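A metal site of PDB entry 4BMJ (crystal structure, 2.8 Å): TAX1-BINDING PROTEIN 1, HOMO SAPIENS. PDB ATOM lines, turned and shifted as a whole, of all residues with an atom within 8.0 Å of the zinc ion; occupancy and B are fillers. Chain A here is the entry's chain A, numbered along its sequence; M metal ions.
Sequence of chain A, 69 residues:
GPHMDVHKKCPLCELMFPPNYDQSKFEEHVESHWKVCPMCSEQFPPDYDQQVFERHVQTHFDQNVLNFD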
ATOM      1  N   LYS A   9      -2.554 -10.442  14.384  1.00  0.00           N
ATOM      2  CA  LYS A   9      -3.248  -9.974  13.200  1.00  0.00           C
ATOM      3  C   LYS A   9      -3.826  -8.597  13.507  1.00  0.00           C
ATOM      4  O   LYS A   9      -4.448  -8.395  14.529  1.00  0.00           O
ATOM      5  CB  LYS A   9      -4.401 -10.935  12.932  1.00  0.00           C
ATOM      6  CG  LYS A   9      -5.048 -10.824  11.592  1.00  0.00           C
ATOM      7  CD  LYS A   9      -4.627 -11.974  10.699  1.00  0.00           C
ATOM      8  CE  LYS A   9      -4.846 -13.291  11.387  1.00  0.00           C
ATOM      9  NZ  LYS A   9      -3.852 -14.290  10.938  1.00  0.00           N
ATOM     10  N   CYS A  10      -3.636  -7.624  12.629  1.00  0.00           N
ATOM     11  CA  CYS A  10      -4.428  -6.420  12.756  1.00  0.00           C
ATOM     12  C   CYS A  10      -5.817  -6.815  12.320  1.00  0.00           C
ATOM     13  O   CYS A  10      -5.983  -7.565  11.369  1.00  0.00           O
ATOM     14  CB  CYS A  10      -3.940  -5.285  11.863  1.00  0.00           C
ATOM     15  SG  CYS A  10      -5.081  -3.856  11.890  1.00  0.00           S
ATOM     16  N   PRO A  11      -6.822  -6.323  13.038  1.00  0.00           N
ATOM     17  CA  PRO A  11      -8.184  -6.650  12.674  1.00  0.00           C
ATOM     18  C   PRO A  11      -8.723  -5.749  11.568  1.00  0.00           C
ATOM     19  O   PRO A  11      -9.649  -6.144  10.885  1.00  0.00           O
ATOM     20  CB  PRO A  11      -8.959  -6.448  13.963  1.00  0.00           C
ATOM     21  CG  PRO A  11      -8.135  -5.524  14.761  1.00  0.00           C
ATOM     22  CD  PRO A  11      -6.729  -5.744  14.394  1.00  0.00           C
ATOM     23  N   LEU A  12      -8.133  -4.578  11.369  1.00  0.00           N
ATOM     24  CA  LEU A  12      -8.675  -3.640  10.382  1.00  0.00           C
ATOM     25  C   LEU A  12      -8.009  -3.676   9.006  1.00  0.00           C
ATOM     26  O   LEU A  12      -8.626  -3.325   8.004  1.00  0.00           O
ATOM     27  CB  LEU A  12      -8.747  -2.218  10.947  1.00  0.00           C
ATOM     28  CG  LEU A  12      -9.675  -2.251  12.185  1.00  0.00           C
ATOM     29  CD1 LEU A  12      -9.685  -0.961  12.991  1.00  0.00           C
ATOM     30  CD2 LEU A  12     -11.104  -2.649  11.770  1.00  0.00           C
ATOM     31  N   CYS A  13      -6.749  -4.124   8.949  1.00  0.00           N
ATOM     32  CA  CYS A  13      -6.035  -4.181   7.675  1.00  0.00           C
ATOM     33  C   CYS A  13      -5.381  -5.535   7.538  1.00  0.00           C
ATOM     34  O   CYS A  13      -5.664  -6.438   8.311  1.00  0.00           O
ATOM     35  CB  CYS A  13      -4.985  -3.096   7.599  1.00  0.00           C
ATOM     36  SG  CYS A  13      -3.643  -3.356   8.738  1.00  0.00           S
ATOM     37  N   GLU A  14      -4.468  -5.685   6.584  1.00  0.00           N
ATOM     38  CA  GLU A  14      -3.909  -6.998   6.313  1.00  0.00           C
ATOM     39  C   GLU A  14      -2.600  -7.263   7.048  1.00  0.00           C
ATOM     40  O   GLU A  14      -2.025  -8.342   6.940  1.00  0.00           O
ATOM     41  CB  GLU A  14      -3.680  -7.164   4.816  1.00  0.00           C
ATOM     42  CG  GLU A  14      -3.786  -8.589   4.368  1.00  0.00           C
ATOM     43  CD  GLU A  14      -5.151  -9.169   4.670  1.00  0.00           C
ATOM     44  OE1 GLU A  14      -6.020  -8.394   5.135  1.00  0.00           O
ATOM     45  OE2 GLU A  14      -5.362 -10.381   4.442  1.00  0.00           O
ATOM     46  N   LEU A  15      -2.127  -6.270   7.790  1.00  0.00           N
ATOM     47  CA  LEU A  15      -0.857  -6.380   8.486  1.00  0.00           C
ATOM     48  C   LEU A  15      -0.833  -7.489   9.556  1.00  0.00           C
ATOM     49  O   LEU A  15      -1.874  -8.000   9.977  1.00  0.00           O
ATOM     50  CB  LEU A  15      -0.452  -5.028   9.085  1.00  0.00           C
ATOM     51  CG  LEU A  15       0.598  -4.212   8.314  1.00  0.00           C
ATOM     52  CD1 LEU A  15       0.605  -4.547   6.804  1.00  0.00           C
ATOM     53  CD2 LEU A  15       0.418  -2.721   8.532  1.00  0.00           C
ATOM     54  N   MET A  16       0.385  -7.849   9.968  1.00  0.00           N
ATOM     55  CA  MET A  16       0.621  -8.852  11.000  1.00  0.00           C
ATOM     56  C   MET A  16       1.880  -8.479  11.780  1.00  0.00           C
ATOM     57  O   MET A  16       2.759  -7.789  11.262  1.00  0.00           O
ATOM     58  CB  MET A  16       0.804 -10.230  10.370  1.00  0.00           C
ATOM     59  CG  MET A  16      -0.394 -10.725   9.580  1.00  0.00           C
ATOM     60  SD  MET A  16      -0.013 -12.087   8.450  1.00  0.00           S
ATOM     61  CE  MET A  16      -1.670 -12.562   7.945  1.00  0.00           C
ATOM     62  N   PHE A  17       1.967  -8.921  13.027  1.00  0.00           N
ATOM     63  CA  PHE A  17       3.082  -8.500  13.868  1.00  0.00           C
ATOM     64  C   PHE A  17       3.794  -9.628  14.607  1.00  0.00           C
ATOM     65  O   PHE A  17       3.240 -10.691  14.837  1.00  0.00           O
ATOM     66  CB  PHE A  17       2.601  -7.451  14.881  1.00  0.00           C
ATOM     67  CG  PHE A  17       2.052  -6.203  14.236  1.00  0.00           C
ATOM     68  CD1 PHE A  17       0.816  -6.209  13.611  1.00  0.00           C
ATOM     69  CD2 PHE A  17       2.788  -5.015  14.264  1.00  0.00           C
ATOM     70  CE1 PHE A  17       0.322  -5.063  13.037  1.00  0.00           C
ATOM     71  CE2 PHE A  17       2.292  -3.866  13.673  1.00  0.00           C
ATOM     72  CZ  PHE A  17       1.052  -3.894  13.056  1.00  0.00           C
ATOM     73  N   PHE A  26       0.822  -1.636  19.166  1.00  0.00           N
ATOM     74  CA  PHE A  26      -0.153  -2.305  18.336  1.00  0.00           C
ATOM     75  C   PHE A  26      -1.516  -1.621  18.447  1.00  0.00           C
ATOM     76  O   PHE A  26      -2.224  -1.425  17.465  1.00  0.00           O
ATOM     77  CB  PHE A  26      -0.263  -3.768  18.749  1.00  0.00           C
ATOM     78  CG  PHE A  26      -1.397  -4.483  18.120  1.00  0.00           C
ATOM     79  CD1 PHE A  26      -1.264  -5.059  16.871  1.00  0.00           C
ATOM     80  CD2 PHE A  26      -2.613  -4.597  18.766  1.00  0.00           C
ATOM     81  CE1 PHE A  26      -2.315  -5.737  16.297  1.00  0.00           C
ATOM     82  CE2 PHE A  26      -3.665  -5.258  18.189  1.00  0.00           C
ATOM     83  CZ  PHE A  26      -3.521  -5.835  16.969  1.00  0.00           C
ATOM     84  N   HIS A  29      -1.326   1.191  16.360  1.00  0.00           N
ATOM     85  CA  HIS A  29      -1.519   0.965  14.941  1.00  0.00           C
ATOM     86  C   HIS A  29      -2.993   0.959  14.646  1.00  0.00           C
ATOM     87  O   HIS A  29      -3.464   1.640  13.742  1.00  0.00           O
ATOM     88  CB  HIS A  29      -0.915  -0.358  14.450  1.00  0.00           C
ATOM     89  CG  HIS A  29      -1.562  -0.855  13.195  1.00  0.00           C
ATOM     90  ND1 HIS A  29      -1.084  -0.526  11.934  1.00  0.00           N
ATOM     91  CD2 HIS A  29      -2.666  -1.615  12.991  1.00  0.00           C
ATOM     92  CE1 HIS A  29      -1.865  -1.090  11.027  1.00  0.00           C
ATOM     93  NE2 HIS A  29      -2.826  -1.769  11.639  1.00  0.00           N
ATOM     94  N   VAL A  30      -3.724   0.162  15.416  1.00  0.00           N
ATOM     95  CA  VAL A  30      -5.128  -0.063  15.152  1.00  0.00           C
ATOM     96  C   VAL A  30      -5.914   1.243  15.120  1.00  0.00           C
ATOM     97  O   VAL A  30      -6.734   1.466  14.234  1.00  0.00           O
ATOM     98  CB  VAL A  30      -5.687  -1.012  16.175  1.00  0.00           C
ATOM     99  CG1 VAL A  30      -7.128  -1.279  15.885  1.00  0.00           C
ATOM    100  CG2 VAL A  30      -4.895  -2.282  16.143  1.00  0.00           C
ATOM    101  N   GLU A  31      -5.622   2.092  16.090  1.00  0.00           N
ATOM    102  CA  GLU A  31      -6.248   3.393  16.208  1.00  0.00           C
ATOM    103  C   GLU A  31      -6.061   4.213  14.943  1.00  0.00           C
ATOM    104  O   GLU A  31      -6.866   5.102  14.665  1.00  0.00           O
ATOM    105  CB  GLU A  31      -5.668   4.151  17.404  1.00  0.00           C
ATOM    106  CG  GLU A  31      -5.983   5.636  17.384  1.00  0.00           C
ATOM    107  CD  GLU A  31      -5.332   6.408  18.532  1.00  0.00           C
ATOM    108  OE1 GLU A  31      -4.092   6.353  18.692  1.00  0.00           O
ATOM    109  OE2 GLU A  31      -6.057   7.092  19.277  1.00  0.00           O
ATOM    110  N   SER A  32      -5.006   3.910  14.175  1.00  0.00           N
ATOM    111  CA  SER A  32      -4.631   4.750  13.062  1.00  0.00           C
ATOM    112  C   SER A  32      -5.529   4.555  11.848  1.00  0.00           C
ATOM    113  O   SER A  32      -5.327   5.213  10.832  1.00  0.00           O
ATOM    114  CB  SER A  32      -3.181   4.494  12.642  1.00  0.00           C
ATOM    115  OG  SER A  32      -3.043   3.272  11.914  1.00  0.00           O
ATOM    116  N   HIS A  33      -6.478   3.617  11.925  1.00  0.00           N
ATOM    117  CA  HIS A  33      -7.445   3.423  10.845  1.00  0.00           C
ATOM    118  C   HIS A  33      -8.756   4.146  11.168  1.00  0.00           C
ATOM    119  O   HIS A  33      -9.555   4.438  10.297  1.00  0.00           O
ATOM    120  CB  HIS A  33      -7.779   1.939  10.615  1.00  0.00           C
ATOM    121  CG  HIS A  33      -6.592   1.068  10.335  1.00  0.00           C
ATOM    122  ND1 HIS A  33      -6.079   0.894   9.067  1.00  0.00           N
ATOM    123  CD2 HIS A  33      -5.885   0.244  11.139  1.00  0.00           C
ATOM    124  CE1 HIS A  33      -5.081   0.020   9.117  1.00  0.00           C
ATOM    125  NE2 HIS A  33      -4.945  -0.384  10.365  1.00  0.00           N
HETATM  126 ZN    ZN M   1      -4.171  -2.395  10.467  1.00  0.00          ZN
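N of Leu 12 sits close to SG of Cys 10 (3.2 Å). The backbone carbonyl oxygen (O) of His 29 lies within hydrogen-bond range of the side-chain hydroxyl (OG) of Ser 32 (2.5 Å). The backbone NH (N) of Cys 10 lies within hydrogen-bond range of the backbone carbonyl oxygen (O) of Leu 15 (3.2 Å). The side-chain sulfur (SG) of Cys 13 sits close to the backbone NH (N) of Leu 15, 3.4 Å away.
The zinc ion is bound by a ring nitrogen (NE2) of His 29, the side-chain sulfur (SG) of Cys 13, a ring nitrogen (NE2) of His 33 and the side-chain sulfur (SG) of Cys 10. The zinc ion has four donor atoms within binding distance.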
